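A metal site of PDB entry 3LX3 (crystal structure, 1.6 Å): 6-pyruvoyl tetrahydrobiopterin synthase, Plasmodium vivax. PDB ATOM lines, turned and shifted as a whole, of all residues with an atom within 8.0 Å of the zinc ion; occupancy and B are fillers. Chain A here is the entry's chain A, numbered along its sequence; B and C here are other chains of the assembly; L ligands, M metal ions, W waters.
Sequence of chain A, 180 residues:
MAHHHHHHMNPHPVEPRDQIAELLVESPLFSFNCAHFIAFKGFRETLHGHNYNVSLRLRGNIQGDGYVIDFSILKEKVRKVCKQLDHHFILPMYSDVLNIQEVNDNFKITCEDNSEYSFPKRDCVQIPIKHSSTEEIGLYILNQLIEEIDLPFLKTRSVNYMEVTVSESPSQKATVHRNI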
ATOM      1  N   CYS A  34      12.308   0.949  18.214  1.00  0.00           N
ATOM      2  CA  CYS A  34      11.857   2.040  19.060  1.00  0.00           C
ATOM      3  C   CYS A  34      10.349   2.108  19.153  1.00  0.00           C
ATOM      4  O   CYS A  34       9.619   1.690  18.230  1.00  0.00           O
ATOM      5  CB  CYS A  34      12.360   3.400  18.541  1.00  0.00           C
ATOM      6  SG  CYS A  34      14.146   3.592  18.733  1.00  0.00           S
ATOM      7  N   ALA A  35       9.889   2.702  20.252  1.00  0.00           N
ATOM      8  CA  ALA A  35       8.502   3.054  20.414  1.00  0.00           C
ATOM      9  C   ALA A  35       8.298   4.542  20.048  1.00  0.00           C
ATOM     10  O   ALA A  35       9.197   5.357  20.205  1.00  0.00           O
ATOM     11  CB  ALA A  35       8.061   2.801  21.866  1.00  0.00           C
ATOM     12  N   HIS A  36       7.098   4.881  19.581  1.00  0.00           N
ATOM     13  CA  HIS A  36       6.781   6.266  19.259  1.00  0.00           C
ATOM     14  C   HIS A  36       5.270   6.424  19.152  1.00  0.00           C
ATOM     15  O   HIS A  36       4.543   5.443  19.121  1.00  0.00           O
ATOM     16  CB  HIS A  36       7.509   6.714  17.973  1.00  0.00           C
ATOM     17  CG  HIS A  36       6.746   6.504  16.701  1.00  0.00           C
ATOM     18  ND1 HIS A  36       6.536   7.527  15.806  1.00  0.00           N
ATOM     19  CD2 HIS A  36       6.211   5.391  16.152  1.00  0.00           C
ATOM     20  CE1 HIS A  36       5.889   7.049  14.757  1.00  0.00           C
ATOM     21  NE2 HIS A  36       5.650   5.755  14.937  1.00  0.00           N
ATOM     22  N   PHE A  37       4.842   7.663  18.979  1.00  0.00           N
ATOM     23  CA  PHE A  37       3.525   7.928  18.391  1.00  0.00           C
ATOM     24  C   PHE A  37       3.581   9.309  17.746  1.00  0.00           C
ATOM     25  O   PHE A  37       4.152  10.273  18.301  1.00  0.00           O
ATOM     26  CB  PHE A  37       2.350   7.776  19.419  1.00  0.00           C
ATOM     27  CG  PHE A  37       2.382   8.725  20.586  1.00  0.00           C
ATOM     28  CD1 PHE A  37       1.772   9.977  20.514  1.00  0.00           C
ATOM     29  CD2 PHE A  37       2.931   8.324  21.785  1.00  0.00           C
ATOM     30  CE1 PHE A  37       1.735  10.804  21.624  1.00  0.00           C
ATOM     31  CE2 PHE A  37       2.930   9.143  22.868  1.00  0.00           C
ATOM     32  CZ  PHE A  37       2.340  10.395  22.781  1.00  0.00           C
ATOM     33  N   ILE A  38       2.907   9.429  16.609  1.00  0.00           N
ATOM     34  CA  ILE A  38       2.724  10.712  15.912  1.00  0.00           C
ATOM     35  C   ILE A  38       1.658  11.535  16.607  1.00  0.00           C
ATOM     36  O   ILE A  38       0.594  11.008  16.956  1.00  0.00           O
ATOM     37  CB  ILE A  38       2.240  10.473  14.446  1.00  0.00           C
ATOM     38  CG1 ILE A  38       3.302   9.732  13.632  1.00  0.00           C
ATOM     39  CG2 ILE A  38       1.807  11.819  13.781  1.00  0.00           C
ATOM     40  CD1 ILE A  38       4.610  10.442  13.452  1.00  0.00           C
ATOM     41  N   GLU A  45      -2.044   9.483  17.593  1.00  0.00           N
ATOM     42  CA  GLU A  45      -2.256   8.031  17.477  1.00  0.00           C
ATOM     43  C   GLU A  45      -1.781   7.320  18.695  1.00  0.00           C
ATOM     44  O   GLU A  45      -1.135   7.929  19.561  1.00  0.00           O
ATOM     45  CB  GLU A  45      -1.541   7.517  16.267  1.00  0.00           C
ATOM     46  CG  GLU A  45      -0.106   7.496  16.403  1.00  0.00           C
ATOM     47  CD  GLU A  45       0.620   7.108  15.107  1.00  0.00           C
ATOM     48  OE1 GLU A  45       0.005   6.526  14.190  1.00  0.00           O
ATOM     49  OE2 GLU A  45       1.825   7.347  15.049  1.00  0.00           O
ATOM     50  N   THR A  46      -2.122   6.044  18.771  1.00  0.00           N
ATOM     51  CA  THR A  46      -1.767   5.192  19.895  1.00  0.00           C
ATOM     52  C   THR A  46      -0.301   4.871  19.889  1.00  0.00           C
ATOM     53  O   THR A  46       0.354   4.789  18.829  1.00  0.00           O
ATOM     54  CB  THR A  46      -2.625   3.939  19.945  1.00  0.00           C
ATOM     55  OG1 THR A  46      -2.578   3.261  18.698  1.00  0.00           O
ATOM     56  CG2 THR A  46      -4.083   4.286  20.291  1.00  0.00           C
ATOM     57  N   LEU A  47       0.245   4.623  21.083  1.00  0.00           N
ATOM     58  CA  LEU A  47       1.608   4.133  21.255  1.00  0.00           C
ATOM     59  C   LEU A  47       1.854   2.825  20.530  1.00  0.00           C
ATOM     60  O   LEU A  47       1.083   1.878  20.660  1.00  0.00           O
ATOM     61  CB  LEU A  47       1.886   3.942  22.762  1.00  0.00           C
ATOM     62  CG  LEU A  47       3.271   3.431  23.147  1.00  0.00           C
ATOM     63  CD1 LEU A  47       4.323   4.462  22.854  1.00  0.00           C
ATOM     64  CD2 LEU A  47       3.263   3.095  24.654  1.00  0.00           C
ATOM     65  N   HIS A  48       2.954   2.782  19.783  1.00  0.00           N
ATOM     66  CA  HIS A  48       3.349   1.558  19.090  1.00  0.00           C
ATOM     67  C   HIS A  48       4.852   1.639  18.829  1.00  0.00           C
ATOM     68  O   HIS A  48       5.553   2.335  19.539  1.00  0.00           O
ATOM     69  CB  HIS A  48       2.494   1.399  17.818  1.00  0.00           C
ATOM     70  CG  HIS A  48       2.732   2.480  16.822  1.00  0.00           C
ATOM     71  ND1 HIS A  48       2.230   3.767  16.954  1.00  0.00           N
ATOM     72  CD2 HIS A  48       3.486   2.486  15.705  1.00  0.00           C
ATOM     73  CE1 HIS A  48       2.685   4.509  15.965  1.00  0.00           C
ATOM     74  NE2 HIS A  48       3.449   3.769  15.174  1.00  0.00           N
ATOM     75  N   GLY A  49       5.355   0.835  17.902  1.00  0.00           N
ATOM     76  CA  GLY A  49       6.770   0.866  17.615  1.00  0.00           C
ATOM     77  C   GLY A  49       7.067   0.229  16.295  1.00  0.00           C
ATOM     78  O   GLY A  49       6.171  -0.215  15.595  1.00  0.00           O
ATOM     79  N   HIS A  50       8.354   0.267  15.968  1.00  0.00           N
ATOM     80  CA  HIS A  50       8.922  -0.132  14.679  1.00  0.00           C
ATOM     81  C   HIS A  50      10.352  -0.596  14.837  1.00  0.00           C
ATOM     82  O   HIS A  50      11.083  -0.153  15.717  1.00  0.00           O
ATOM     83  CB  HIS A  50       8.960   1.066  13.759  1.00  0.00           C
ATOM     84  CG  HIS A  50       7.635   1.680  13.485  1.00  0.00           C
ATOM     85  ND1 HIS A  50       6.636   1.027  12.792  1.00  0.00           N
ATOM     86  CD2 HIS A  50       7.118   2.886  13.828  1.00  0.00           C
ATOM     87  CE1 HIS A  50       5.576   1.803  12.725  1.00  0.00           C
ATOM     88  NE2 HIS A  50       5.834   2.942  13.337  1.00  0.00           N
ATOM     89  N   TYR A  52      12.997   0.511  12.947  1.00  0.00           N
ATOM     90  CA  TYR A  52      13.433   1.498  11.976  1.00  0.00           C
ATOM     91  C   TYR A  52      14.715   1.061  11.322  1.00  0.00           C
ATOM     92  O   TYR A  52      15.590   0.459  11.956  1.00  0.00           O
ATOM     93  CB  TYR A  52      13.685   2.830  12.646  1.00  0.00           C
ATOM     94  CG  TYR A  52      12.466   3.617  13.115  1.00  0.00           C
ATOM     95  CD1 TYR A  52      11.840   4.526  12.281  1.00  0.00           C
ATOM     96  CD2 TYR A  52      11.944   3.458  14.393  1.00  0.00           C
ATOM     97  CE1 TYR A  52      10.752   5.314  12.710  1.00  0.00           C
ATOM     98  CE2 TYR A  52      10.844   4.209  14.806  1.00  0.00           C
ATOM     99  CZ  TYR A  52      10.238   5.114  13.970  1.00  0.00           C
ATOM    100  OH  TYR A  52       9.155   5.814  14.454  1.00  0.00           O
ATOM    101  N   SER A 132       7.667  12.758  15.716  1.00  0.00           N
ATOM    102  CA  SER A 132       8.415  11.547  15.410  1.00  0.00           C
ATOM    103  C   SER A 132       8.019  10.890  14.067  1.00  0.00           C
ATOM    104  O   SER A 132       7.746   9.675  13.982  1.00  0.00           O
ATOM    105  CB  SER A 132       8.349  10.565  16.582  1.00  0.00           C
ATOM    106  OG  SER A 132       6.997  10.240  16.883  1.00  0.00           O
ATOM    107  N   SER A 133       7.997  11.739  13.034  1.00  0.00           N
ATOM    108  CA  SER A 133       7.747  11.253  11.689  1.00  0.00           C
ATOM    109  C   SER A 133       9.035  10.728  11.090  1.00  0.00           C
ATOM    110  O   SER A 133      10.161  11.088  11.474  1.00  0.00           O
ATOM    111  CB  SER A 133       7.173  12.346  10.816  1.00  0.00           C
ATOM    112  OG  SER A 133       8.095  13.428  10.631  1.00  0.00           O
ATOM    113  N   THR A 134       8.843   9.896  10.067  1.00  0.00           N
ATOM    114  CA  THR A 134       9.960   9.365   9.355  1.00  0.00           C
ATOM    115  C   THR A 134      10.869  10.436   8.760  1.00  0.00           C
ATOM    116  O   THR A 134      12.081  10.343   8.832  1.00  0.00           O
ATOM    117  CB  THR A 134       9.397   8.399   8.293  1.00  0.00           C
ATOM    118  OG1 THR A 134       8.465   7.482   8.898  1.00  0.00           O
ATOM    119  CG2 THR A 134      10.516   7.597   7.643  1.00  0.00           C
ATOM    120  N   GLU A 168      10.145   3.431   8.680  1.00  0.00           N
ATOM    121  CA  GLU A 168       9.444   2.910   9.834  1.00  0.00           C
ATOM    122  C   GLU A 168       9.227   1.416   9.595  1.00  0.00           C
ATOM    123  O   GLU A 168       9.304   0.644  10.497  1.00  0.00           O
ATOM    124  CB  GLU A 168       8.013   3.464   9.982  1.00  0.00           C
ATOM    125  CG  GLU A 168       7.760   4.695  10.805  1.00  0.00           C
ATOM    126  CD  GLU A 168       6.248   5.027  10.839  1.00  0.00           C
ATOM    127  OE1 GLU A 168       5.500   4.373  10.079  1.00  0.00           O
ATOM    128  OE2 GLU A 168       5.803   5.874  11.637  1.00  0.00           O
ATOM    129  N   SER A 169       8.899   1.060   8.359  1.00  0.00           N
ATOM    130  CA  SER A 169       8.675  -0.330   7.948  1.00  0.00           C
ATOM    131  C   SER A 169       9.156  -0.337   6.502  1.00  0.00           C
ATOM    132  O   SER A 169       9.233   0.741   5.883  1.00  0.00           O
ATOM    133  CB  SER A 169       7.196  -0.675   8.099  1.00  0.00           C
ATOM    134  OG  SER A 169       6.436  -0.055   7.102  1.00  0.00           O
ATOM    135  N   GLN A 172       7.471   1.932   3.722  1.00  0.00           N
ATOM    136  CA  GLN A 172       7.351   3.375   3.696  1.00  0.00           C
ATOM    137  C   GLN A 172       8.615   4.068   4.192  1.00  0.00           C
ATOM    138  O   GLN A 172       9.025   3.875   5.351  1.00  0.00           O
ATOM    139  CB  GLN A 172       6.146   3.850   4.472  1.00  0.00           C
ATOM    140  CG  GLN A 172       5.947   3.291   5.814  1.00  0.00           C
ATOM    141  CD  GLN A 172       4.608   3.726   6.438  1.00  0.00           C
ATOM    142  OE1 GLN A 172       3.540   3.404   5.938  1.00  0.00           O
ATOM    143  NE2 GLN A 172       4.701   4.487   7.556  1.00  0.00           N
ATOM    144  N   ASN B  33       2.675  -3.614  14.386  1.00  0.00           N
ATOM    145  CA  ASN B  33       3.693  -2.701  14.795  1.00  0.00           C
ATOM    146  C   ASN B  33       3.368  -2.213  16.192  1.00  0.00           C
ATOM    147  O   ASN B  33       2.379  -1.504  16.409  1.00  0.00           O
ATOM    148  CB  ASN B  33       3.718  -1.556  13.800  1.00  0.00           C
ATOM    149  CG  ASN B  33       4.034  -2.016  12.361  1.00  0.00           C
ATOM    150  OD1 ASN B  33       4.408  -3.170  12.096  1.00  0.00           O
ATOM    151  ND2 ASN B  33       3.796  -1.121  11.413  1.00  0.00           N
ATOM    152  N   ASN B  51       8.250  -3.983  14.275  1.00  0.00           N
ATOM    153  CA  ASN B  51       7.330  -4.412  13.268  1.00  0.00           C
ATOM    154  C   ASN B  51       7.301  -5.930  13.336  1.00  0.00           C
ATOM    155  O   ASN B  51       8.114  -6.604  12.716  1.00  0.00           O
ATOM    156  CB  ASN B  51       7.826  -3.978  11.898  1.00  0.00           C
ATOM    157  CG  ASN B  51       8.023  -2.500  11.764  1.00  0.00           C
ATOM    158  OD1 ASN B  51       7.211  -1.712  12.240  1.00  0.00           O
ATOM    159  ND2 ASN B  51       9.133  -2.093  11.111  1.00  0.00           N
ATOM    160  N   HIS B  87      -0.449  -1.543  16.380  1.00  0.00           N
ATOM    161  CA  HIS B  87      -0.552  -0.149  16.831  1.00  0.00           C
ATOM    162  C   HIS B  87      -0.935  -0.047  18.283  1.00  0.00           C
ATOM    163  O   HIS B  87      -1.689   0.799  18.690  1.00  0.00           O
ATOM    164  CB  HIS B  87      -1.480   0.724  15.981  1.00  0.00           C
ATOM    165  CG  HIS B  87      -0.736   1.597  15.041  1.00  0.00           C
ATOM    166  ND1 HIS B  87      -0.724   2.967  15.134  1.00  0.00           N
ATOM    167  CD2 HIS B  87       0.100   1.257  14.031  1.00  0.00           C
ATOM    168  CE1 HIS B  87       0.054   3.448  14.175  1.00  0.00           C
ATOM    169  NE2 HIS B  87       0.557   2.441  13.493  1.00  0.00           N
ATOM    170  N   TYR C  67       4.782  15.731   7.963  1.00  0.00           N
ATOM    171  CA  TYR C  67       4.790  14.916   6.767  1.00  0.00           C
ATOM    172  C   TYR C  67       4.951  15.740   5.505  1.00  0.00           C
ATOM    173  O   TYR C  67       4.497  16.890   5.472  1.00  0.00           O
ATOM    174  CB  TYR C  67       3.430  14.217   6.592  1.00  0.00           C
ATOM    175  CG  TYR C  67       2.971  13.243   7.684  1.00  0.00           C
ATOM    176  CD1 TYR C  67       3.826  12.668   8.597  1.00  0.00           C
ATOM    177  CD2 TYR C  67       1.623  12.956   7.771  1.00  0.00           C
ATOM    178  CE1 TYR C  67       3.350  11.781   9.549  1.00  0.00           C
ATOM    179  CE2 TYR C  67       1.143  12.062   8.705  1.00  0.00           C
ATOM    180  CZ  TYR C  67       2.001  11.479   9.577  1.00  0.00           C
ATOM    181  OH  TYR C  67       1.500  10.591  10.491  1.00  0.00           O
HETATM  182  N1  LIG L   1       3.207   9.616   6.701  1.00  0.00           N
HETATM  183  C1  LIG L   1       4.422  10.196   6.539  1.00  0.00           C
HETATM  184  N2  LIG L   1       4.666  10.996   5.488  1.00  0.00           N
HETATM  185  N3  LIG L   1       5.441  10.001   7.508  1.00  0.00           N
HETATM  186  C2  LIG L   1       5.272   9.204   8.574  1.00  0.00           C
HETATM  187  O1  LIG L   1       6.226   9.044   9.367  1.00  0.00           O
HETATM  188  N4  LIG L   1       3.752   7.763   9.749  1.00  0.00           N
HETATM  189  C3  LIG L   1       2.513   7.192   9.869  1.00  0.00           C
HETATM  190  O2  LIG L   1       2.284   6.458  10.826  1.00  0.00           O
HETATM  191  C4  LIG L   1       1.497   7.479   8.908  1.00  0.00           C
HETATM  192  N5  LIG L   1       1.797   8.281   7.887  1.00  0.00           N
HETATM  193  C5  LIG L   1       4.022   8.589   8.692  1.00  0.00           C
HETATM  194  C6  LIG L   1       3.015   8.817   7.752  1.00  0.00           C
HETATM  195 ZN    ZN M   1       4.552   4.586  13.581  1.00  0.00          ZN
HETATM  196  O   HOH W   1       3.312   6.169  13.202  1.00  0.00           O
HETATM  197  O   HOH W   2       3.298   3.723  12.018  1.00  0.00           O
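The zinc ion is bound by water W1, a ring nitrogen (NE2) of His 50, a ring nitrogen (NE2) of His 36, a ring nitrogen (NE2) of His 48 and water W2. The zinc ion has five donor atoms within binding distance. Slightly farther from the zinc ion lies the side-chain carboxylate (OE2) of Glu 168 (2.6 Å).
The side-chain carboxylate of Glu 168 is in hydrogen-bond range of the side-chain amide nitrogen of Gln 172 (2.6 Å). The backbone carbonyl oxygen (O) of Thr 46 is in hydrogen-bond range of a ring nitrogen (ND1) of His 48, at 2.8 Å. The backbone carbonyl oxygen of Glu 168 lies within hydrogen-bond range of the side-chain amide nitrogen of Asn 51 of chain B, at 2.8 Å. The side-chain carboxylate (OE2) of Glu 168 lies close to a ring nitrogen (NE2) of His 50 (3.4 Å). A ring nitrogen (ND1) of His 36 sits at hydrogen-bond distance from the side-chain hydroxyl (OG) of Ser 132 (3.0 Å). A ring nitrogen (ND1) of His 50 sits at hydrogen-bond distance from the side-chain amide oxygen of Asn 51 of chain B (2.9 Å). A ring nitrogen (ND1) of His 36 sits close to the side-chain hydroxyl (OH) of Tyr 52, 3.4 Å away. A ring nitrogen (NE2) of His 36 lies close to the side-chain carboxylate (OE2) of Glu 168 (3.3 Å).
The backbone NH (N) of Thr 134 lies within hydrogen-bond range of an oxygen (O1) of the ligand (2.8 Å). The side-chain carboxylate (OE2) of Glu 168 sits at hydrogen-bond distance from a nitrogen (N4) of the ligand, at 3.4 Å. An oxygen (O1) of the ligand sits at hydrogen-bond distance from the side-chain hydroxyl (OG1) of Thr 134 (2.8 Å). OH of Tyr 67 of chain C lies close to N5 of the ligand (3.5 Å).
Water W2 lies within hydrogen-bond range of OE1 of Glu 168 (3.0 Å), O2 of the ligand (3.2 Å) and NE2 of His 87 of chain B (3.4 Å).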
